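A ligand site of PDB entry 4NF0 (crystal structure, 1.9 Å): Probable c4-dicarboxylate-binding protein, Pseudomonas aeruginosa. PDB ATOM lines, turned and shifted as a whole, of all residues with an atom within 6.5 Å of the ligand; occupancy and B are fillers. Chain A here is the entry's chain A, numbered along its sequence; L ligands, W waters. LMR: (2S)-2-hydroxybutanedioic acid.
The side-chain hydroxyl of Tyr 237 sits at hydrogen-bond distance from an oxygen (O4B) of the ligand (2.4 Å). NZ of Lys 42 lies within salt-bridge range of O4A of the ligand, 2.6 Å away. NZ of Lys 95 is in salt-bridge range of O1A of the ligand, at 2.7 Å. The guanidinium group (NH1) of Arg 170 is in salt-bridge range of an oxygen (O1B) of the ligand (2.8 Å). The side-chain amide oxygen of Gln 172 lies within hydrogen-bond range of an oxygen (O2) of the ligand (2.8 Å). An oxygen (O1B) of the ligand lies within hydrogen-bond range of the side-chain amide nitrogen of Asn 210, at 2.9 Å. O4B of the ligand is in hydrogen-bond range of ND2 of Asn 214 (2.9 Å).
The side-chain amide nitrogen of Asn 147 is in hydrogen-bond range of the side-chain hydroxyl of Tyr 237, at 2.9 Å. NZ of Lys 42 lies within hydrogen-bond range of O of Ala 90 (2.7 Å). The side-chain carboxylate (OD1) of Asp 74 is in salt-bridge range of the side-chain amino group (NZ) of Lys 95, 3.0 Å away. OE1 of Gln 172 lies within hydrogen-bond range of OG of Ser 92 (2.6 Å). The side-chain amide oxygen (OD1) of Asn 210 sits at hydrogen-bond distance from the side-chain amide nitrogen (ND2) of Asn 214 (2.9 Å). N of Asn 214 sits at hydrogen-bond distance from OG1 of Thr 211. OD2 of Asp 74 is in hydrogen-bond range of N of Tyr 193 (3.0 Å). O of Tyr 193 is in hydrogen-bond range of NE2 of Gln 218, 3.0 Å away.
Asp 74 touches the ligand. CB of Ser 92 touches O2 of the ligand (3.5 Å). CD1 of Tyr 193 touches O1B of the ligand, 3.6 Å away. Leu 235 touches the ligand (CD2 to O4B, 3.7 Å). Of the 25 residues printed, 11 come within 4 Å of the ligand.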
ATOM      1  N   VAL A  35      23.595 -30.446  19.760  1.00  0.00           N
ATOM      2  CA  VAL A  35      22.845 -29.214  19.957  1.00  0.00           C
ATOM      3  C   VAL A  35      22.889 -28.270  18.749  1.00  0.00           C
ATOM      4  O   VAL A  35      22.263 -27.211  18.776  1.00  0.00           O
ATOM      5  CB  VAL A  35      23.333 -28.449  21.221  1.00  0.00           C
ATOM      6  CG1 VAL A  35      23.220 -29.327  22.457  1.00  0.00           C
ATOM      7  CG2 VAL A  35      24.766 -27.930  21.038  1.00  0.00           C
ATOM      8  N   VAL A  36      23.584 -28.676  17.695  1.00  0.00           N
ATOM      9  CA  VAL A  36      23.685 -27.819  16.510  1.00  0.00           C
ATOM     10  C   VAL A  36      22.998 -28.440  15.285  1.00  0.00           C
ATOM     11  O   VAL A  36      22.359 -29.488  15.379  1.00  0.00           O
ATOM     12  CB  VAL A  36      25.173 -27.504  16.176  1.00  0.00           C
ATOM     13  CG1 VAL A  36      25.827 -26.813  17.360  1.00  0.00           C
ATOM     14  CG2 VAL A  36      25.926 -28.765  15.819  1.00  0.00           C
ATOM     15  N   LYS A  42      30.208 -31.142  13.362  1.00  0.00           N
ATOM     16  CA  LYS A  42      29.701 -32.181  14.256  1.00  0.00           C
ATOM     17  C   LYS A  42      28.477 -32.873  13.663  1.00  0.00           C
ATOM     18  O   LYS A  42      28.355 -34.092  13.730  1.00  0.00           O
ATOM     19  CB  LYS A  42      29.371 -31.583  15.635  1.00  0.00           C
ATOM     20  CG  LYS A  42      28.636 -32.540  16.582  1.00  0.00           C
ATOM     21  CD  LYS A  42      27.951 -31.795  17.732  1.00  0.00           C
ATOM     22  CE  LYS A  42      28.854 -30.770  18.368  1.00  0.00           C
ATOM     23  NZ  LYS A  42      28.513 -30.430  19.794  1.00  0.00           N
ATOM     24  N   ASP A  74      21.910 -28.687  25.794  1.00  0.00           N
ATOM     25  CA  ASP A  74      23.260 -28.445  26.321  1.00  0.00           C
ATOM     26  C   ASP A  74      23.396 -28.787  27.812  1.00  0.00           C
ATOM     27  O   ASP A  74      24.326 -29.490  28.212  1.00  0.00           O
ATOM     28  CB  ASP A  74      23.621 -26.981  26.088  1.00  0.00           C
ATOM     29  CG  ASP A  74      25.036 -26.788  25.593  1.00  0.00           C
ATOM     30  OD1 ASP A  74      25.670 -27.785  25.171  1.00  0.00           O
ATOM     31  OD2 ASP A  74      25.502 -25.631  25.600  1.00  0.00           O
ATOM     32  N   ALA A  90      28.782 -35.538  21.247  1.00  0.00           N
ATOM     33  CA  ALA A  90      30.058 -34.945  20.856  1.00  0.00           C
ATOM     34  C   ALA A  90      30.128 -33.574  21.521  1.00  0.00           C
ATOM     35  O   ALA A  90      29.638 -32.593  20.983  1.00  0.00           O
ATOM     36  CB  ALA A  90      30.196 -34.846  19.349  1.00  0.00           C
ATOM     37  N   THR A  91      30.722 -33.540  22.700  1.00  0.00           N
ATOM     38  CA  THR A  91      30.582 -32.417  23.613  1.00  0.00           C
ATOM     39  C   THR A  91      31.863 -31.592  23.664  1.00  0.00           C
ATOM     40  O   THR A  91      32.967 -32.160  23.667  1.00  0.00           O
ATOM     41  CB  THR A  91      30.205 -32.921  25.032  1.00  0.00           C
ATOM     42  OG1 THR A  91      28.936 -33.602  24.973  1.00  0.00           O
ATOM     43  CG2 THR A  91      30.107 -31.774  26.027  1.00  0.00           C
ATOM     44  N   SER A  92      31.710 -30.271  23.671  1.00  0.00           N
ATOM     45  CA  SER A  92      32.859 -29.371  23.756  1.00  0.00           C
ATOM     46  C   SER A  92      33.738 -29.700  24.949  1.00  0.00           C
ATOM     47  O   SER A  92      33.241 -30.011  26.030  1.00  0.00           O
ATOM     48  CB  SER A  92      32.393 -27.910  23.861  1.00  0.00           C
ATOM     49  OG  SER A  92      33.508 -27.058  23.987  1.00  0.00           O
ATOM     50  N   LYS A  95      33.270 -28.108  28.369  1.00  0.00           N
ATOM     51  CA  LYS A  95      32.098 -28.372  29.209  1.00  0.00           C
ATOM     52  C   LYS A  95      32.223 -29.515  30.208  1.00  0.00           C
ATOM     53  O   LYS A  95      31.232 -29.928  30.801  1.00  0.00           O
ATOM     54  CB  LYS A  95      30.880 -28.618  28.295  1.00  0.00           C
ATOM     55  CG  LYS A  95      30.398 -27.345  27.584  1.00  0.00           C
ATOM     56  CD  LYS A  95      29.406 -27.616  26.459  1.00  0.00           C
ATOM     57  CE  LYS A  95      29.117 -26.287  25.704  1.00  0.00           C
ATOM     58  NZ  LYS A  95      28.309 -26.500  24.473  1.00  0.00           N
ATOM     59  N   ASN A 147      36.219 -28.448  15.639  1.00  0.00           N
ATOM     60  CA  ASN A 147      35.312 -27.571  14.933  1.00  0.00           C
ATOM     61  C   ASN A 147      36.146 -26.529  14.200  1.00  0.00           C
ATOM     62  O   ASN A 147      36.212 -26.517  12.976  1.00  0.00           O
ATOM     63  CB  ASN A 147      34.311 -26.929  15.892  1.00  0.00           C
ATOM     64  CG  ASN A 147      33.291 -26.059  15.181  1.00  0.00           C
ATOM     65  OD1 ASN A 147      33.640 -25.214  14.352  1.00  0.00           O
ATOM     66  ND2 ASN A 147      32.019 -26.241  15.517  1.00  0.00           N
ATOM     67  N   ARG A 170      29.117 -13.891  26.288  1.00  0.00           N
ATOM     68  CA  ARG A 170      28.626 -15.254  26.535  1.00  0.00           C
ATOM     69  C   ARG A 170      29.755 -16.236  26.323  1.00  0.00           C
ATOM     70  O   ARG A 170      30.467 -16.171  25.320  1.00  0.00           O
ATOM     71  CB  ARG A 170      27.459 -15.627  25.626  1.00  0.00           C
ATOM     72  CG  ARG A 170      26.973 -17.078  25.805  1.00  0.00           C
ATOM     73  CD  ARG A 170      27.698 -18.080  24.885  1.00  0.00           C
ATOM     74  NE  ARG A 170      27.441 -19.472  25.304  1.00  0.00           N
ATOM     75  CZ  ARG A 170      27.672 -20.531  24.539  1.00  0.00           C
ATOM     76  NH1 ARG A 170      28.119 -20.386  23.308  1.00  0.00           N
ATOM     77  NH2 ARG A 170      27.415 -21.752  25.006  1.00  0.00           N
ATOM     78  N   ILE A 171      29.909 -17.153  27.274  1.00  0.00           N
ATOM     79  CA  ILE A 171      30.853 -18.246  27.124  1.00  0.00           C
ATOM     80  C   ILE A 171      30.169 -19.571  27.413  1.00  0.00           C
ATOM     81  O   ILE A 171      29.095 -19.615  28.007  1.00  0.00           O
ATOM     82  CB  ILE A 171      32.053 -18.085  28.069  1.00  0.00           C
ATOM     83  CG1 ILE A 171      31.559 -18.005  29.517  1.00  0.00           C
ATOM     84  CG2 ILE A 171      32.883 -16.863  27.637  1.00  0.00           C
ATOM     85  CD1 ILE A 171      32.619 -18.261  30.578  1.00  0.00           C
ATOM     86  N   GLN A 172      30.817 -20.657  26.988  1.00  0.00           N
ATOM     87  CA  GLN A 172      30.473 -21.994  27.473  1.00  0.00           C
ATOM     88  C   GLN A 172      30.797 -22.095  28.966  1.00  0.00           C
ATOM     89  O   GLN A 172      31.609 -21.324  29.476  1.00  0.00           O
ATOM     90  CB  GLN A 172      31.246 -23.050  26.683  1.00  0.00           C
ATOM     91  CG  GLN A 172      30.977 -23.044  25.194  1.00  0.00           C
ATOM     92  CD  GLN A 172      32.095 -23.684  24.411  1.00  0.00           C
ATOM     93  OE1 GLN A 172      32.044 -24.870  24.086  1.00  0.00           O
ATOM     94  NE2 GLN A 172      33.134 -22.906  24.115  1.00  0.00           N
ATOM     95  N   PRO A 173      30.164 -23.039  29.683  1.00  0.00           N
ATOM     96  CA  PRO A 173      30.309 -23.029  31.150  1.00  0.00           C
ATOM     97  C   PRO A 173      31.666 -23.517  31.626  1.00  0.00           C
ATOM     98  O   PRO A 173      31.751 -24.582  32.242  1.00  0.00           O
ATOM     99  CB  PRO A 173      29.184 -23.958  31.615  1.00  0.00           C
ATOM    100  CG  PRO A 173      28.960 -24.884  30.468  1.00  0.00           C
ATOM    101  CD  PRO A 173      29.238 -24.080  29.215  1.00  0.00           C
ATOM    102  N   LEU A 191      26.374 -19.455  29.640  1.00  0.00           N
ATOM    103  CA  LEU A 191      25.079 -19.751  29.040  1.00  0.00           C
ATOM    104  C   LEU A 191      25.196 -20.927  28.084  1.00  0.00           C
ATOM    105  O   LEU A 191      26.269 -21.195  27.532  1.00  0.00           O
ATOM    106  CB  LEU A 191      24.542 -18.527  28.287  1.00  0.00           C
ATOM    107  CG  LEU A 191      24.168 -17.276  29.069  1.00  0.00           C
ATOM    108  CD1 LEU A 191      23.783 -16.169  28.114  1.00  0.00           C
ATOM    109  CD2 LEU A 191      23.001 -17.592  30.022  1.00  0.00           C
ATOM    110  N   SER A 192      24.082 -21.617  27.860  1.00  0.00           N
ATOM    111  CA  SER A 192      24.062 -22.732  26.922  1.00  0.00           C
ATOM    112  C   SER A 192      24.144 -22.197  25.498  1.00  0.00           C
ATOM    113  O   SER A 192      23.941 -21.002  25.277  1.00  0.00           O
ATOM    114  CB  SER A 192      22.800 -23.571  27.097  1.00  0.00           C
ATOM    115  OG  SER A 192      21.700 -22.891  26.524  1.00  0.00           O
ATOM    116  N   TYR A 193      24.439 -23.082  24.539  1.00  0.00           N
ATOM    117  CA  TYR A 193      24.476 -22.693  23.137  1.00  0.00           C
ATOM    118  C   TYR A 193      23.171 -21.991  22.731  1.00  0.00           C
ATOM    119  O   TYR A 193      23.211 -20.918  22.107  1.00  0.00           O
ATOM    120  CB  TYR A 193      24.747 -23.913  22.252  1.00  0.00           C
ATOM    121  CG  TYR A 193      24.563 -23.626  20.774  1.00  0.00           C
ATOM    122  CD1 TYR A 193      25.577 -23.054  20.019  1.00  0.00           C
ATOM    123  CD2 TYR A 193      23.358 -23.919  20.140  1.00  0.00           C
ATOM    124  CE1 TYR A 193      25.396 -22.775  18.671  1.00  0.00           C
ATOM    125  CE2 TYR A 193      23.168 -23.636  18.792  1.00  0.00           C
ATOM    126  CZ  TYR A 193      24.190 -23.070  18.060  1.00  0.00           C
ATOM    127  OH  TYR A 193      23.992 -22.804  16.718  1.00  0.00           O
ATOM    128  N   ALA A 194      22.026 -22.565  23.089  1.00  0.00           N
ATOM    129  CA  ALA A 194      20.733 -22.058  22.620  1.00  0.00           C
ATOM    130  C   ALA A 194      20.242 -20.800  23.339  1.00  0.00           C
ATOM    131  O   ALA A 194      19.370 -20.098  22.826  1.00  0.00           O
ATOM    132  CB  ALA A 194      19.688 -23.148  22.715  1.00  0.00           C
ATOM    133  N   THR A 196      22.028 -18.166  23.958  1.00  0.00           N
ATOM    134  CA  THR A 196      22.927 -17.049  23.638  1.00  0.00           C
ATOM    135  C   THR A 196      22.224 -15.897  22.921  1.00  0.00           C
ATOM    136  O   THR A 196      22.405 -14.735  23.281  1.00  0.00           O
ATOM    137  CB  THR A 196      24.129 -17.534  22.782  1.00  0.00           C
ATOM    138  OG1 THR A 196      24.872 -18.526  23.505  1.00  0.00           O
ATOM    139  CG2 THR A 196      25.064 -16.364  22.430  1.00  0.00           C
ATOM    140  N   GLU A 209      32.386 -15.530  22.059  1.00  0.00           N
ATOM    141  CA  GLU A 209      33.444 -16.179  21.298  1.00  0.00           C
ATOM    142  C   GLU A 209      32.873 -17.441  20.669  1.00  0.00           C
ATOM    143  O   GLU A 209      32.137 -18.181  21.330  1.00  0.00           O
ATOM    144  CB  GLU A 209      34.647 -16.516  22.209  1.00  0.00           C
ATOM    145  CG  GLU A 209      34.283 -17.364  23.456  1.00  0.00           C
ATOM    146  CD  GLU A 209      35.497 -18.032  24.106  1.00  0.00           C
ATOM    147  OE1 GLU A 209      36.625 -17.528  23.965  1.00  0.00           O
ATOM    148  OE2 GLU A 209      35.318 -19.068  24.776  1.00  0.00           O
ATOM    149  N   ASN A 210      33.178 -17.680  19.394  1.00  0.00           N
ATOM    150  CA  ASN A 210      32.808 -18.936  18.749  1.00  0.00           C
ATOM    151  C   ASN A 210      33.389 -19.063  17.349  1.00  0.00           C
ATOM    152  O   ASN A 210      33.977 -18.111  16.805  1.00  0.00           O
ATOM    153  CB  ASN A 210      31.288 -19.108  18.698  1.00  0.00           C
ATOM    154  CG  ASN A 210      30.862 -20.477  19.214  1.00  0.00           C
ATOM    155  OD1 ASN A 210      31.465 -21.492  18.825  1.00  0.00           O
ATOM    156  ND2 ASN A 210      29.871 -20.512  20.104  1.00  0.00           N
ATOM    157  N   THR A 211      33.285 -20.262  16.779  1.00  0.00           N
ATOM    158  CA  THR A 211      33.760 -20.474  15.421  1.00  0.00           C
ATOM    159  C   THR A 211      32.787 -19.831  14.462  1.00  0.00           C
ATOM    160  O   THR A 211      31.648 -19.550  14.849  1.00  0.00           O
ATOM    161  CB  THR A 211      33.881 -21.959  15.080  1.00  0.00           C
ATOM    162  OG1 THR A 211      32.579 -22.560  15.126  1.00  0.00           O
ATOM    163  CG2 THR A 211      34.791 -22.663  16.077  1.00  0.00           C
ATOM    164  N   ASN A 214      29.419 -21.614  14.250  1.00  0.00           N
ATOM    165  CA  ASN A 214      28.483 -21.395  15.344  1.00  0.00           C
ATOM    166  C   ASN A 214      27.973 -19.960  15.421  1.00  0.00           C
ATOM    167  O   ASN A 214      26.842 -19.730  15.866  1.00  0.00           O
ATOM    168  CB  ASN A 214      29.118 -21.789  16.675  1.00  0.00           C
ATOM    169  CG  ASN A 214      29.079 -23.294  16.924  1.00  0.00           C
ATOM    170  OD1 ASN A 214      28.365 -24.031  16.231  1.00  0.00           O
ATOM    171  ND2 ASN A 214      29.831 -23.743  17.929  1.00  0.00           N
ATOM    172  N   GLN A 218      24.016 -19.537  15.417  1.00  0.00           N
ATOM    173  CA  GLN A 218      23.291 -18.883  16.497  1.00  0.00           C
ATOM    174  C   GLN A 218      22.466 -17.722  15.983  1.00  0.00           C
ATOM    175  O   GLN A 218      21.587 -17.212  16.695  1.00  0.00           O
ATOM    176  CB  GLN A 218      24.254 -18.390  17.582  1.00  0.00           C
ATOM    177  CG  GLN A 218      24.834 -19.513  18.433  1.00  0.00           C
ATOM    178  CD  GLN A 218      25.672 -19.023  19.598  1.00  0.00           C
ATOM    179  OE1 GLN A 218      26.478 -18.092  19.470  1.00  0.00           O
ATOM    180  NE2 GLN A 218      25.519 -19.682  20.744  1.00  0.00           N
ATOM    181  N   LEU A 235      37.763 -24.538  19.449  1.00  0.00           N
ATOM    182  CA  LEU A 235      36.538 -25.239  19.806  1.00  0.00           C
ATOM    183  C   LEU A 235      36.679 -26.665  19.315  1.00  0.00           C
ATOM    184  O   LEU A 235      36.768 -26.914  18.113  1.00  0.00           O
ATOM    185  CB  LEU A 235      35.293 -24.587  19.197  1.00  0.00           C
ATOM    186  CG  LEU A 235      34.016 -25.411  19.390  1.00  0.00           C
ATOM    187  CD1 LEU A 235      33.692 -25.608  20.847  1.00  0.00           C
ATOM    188  CD2 LEU A 235      32.852 -24.712  18.670  1.00  0.00           C
ATOM    189  N   TYR A 237      35.727 -31.063  20.274  1.00  0.00           N
ATOM    190  CA  TYR A 237      34.794 -31.942  20.975  1.00  0.00           C
ATOM    191  C   TYR A 237      35.444 -33.255  21.371  1.00  0.00           C
ATOM    192  O   TYR A 237      36.363 -33.720  20.703  1.00  0.00           O
ATOM    193  CB  TYR A 237      33.589 -32.277  20.089  1.00  0.00           C
ATOM    194  CG  TYR A 237      32.895 -31.128  19.403  1.00  0.00           C
ATOM    195  CD1 TYR A 237      32.200 -30.170  20.132  1.00  0.00           C
ATOM    196  CD2 TYR A 237      32.909 -31.027  18.017  1.00  0.00           C
ATOM    197  CE1 TYR A 237      31.558 -29.120  19.495  1.00  0.00           C
ATOM    198  CE2 TYR A 237      32.260 -29.993  17.365  1.00  0.00           C
ATOM    199  CZ  TYR A 237      31.595 -29.041  18.113  1.00  0.00           C
ATOM    200  OH  TYR A 237      30.946 -28.005  17.492  1.00  0.00           O
HETATM  201  C1  LMR L   1      28.715 -23.709  22.308  1.00  0.00           C
HETATM  202  O1A LMR L   1      28.227 -23.999  23.423  1.00  0.00           O
HETATM  203  O1B LMR L   1      28.663 -22.592  21.745  1.00  0.00           O
HETATM  204  C2  LMR L   1      29.399 -24.839  21.522  1.00  0.00           C
HETATM  205  O2  LMR L   1      30.024 -25.765  22.417  1.00  0.00           O
HETATM  206  C3  LMR L   1      28.343 -25.544  20.648  1.00  0.00           C
HETATM  207  C4  LMR L   1      28.982 -26.742  19.933  1.00  0.00           C
HETATM  208  O4A LMR L   1      28.732 -27.875  20.422  1.00  0.00           O
HETATM  209  O4B LMR L   1      29.663 -26.507  18.908  1.00  0.00           O
HETATM  210  O   HOH W   1      29.127 -28.883  22.851  1.00  0.00           O
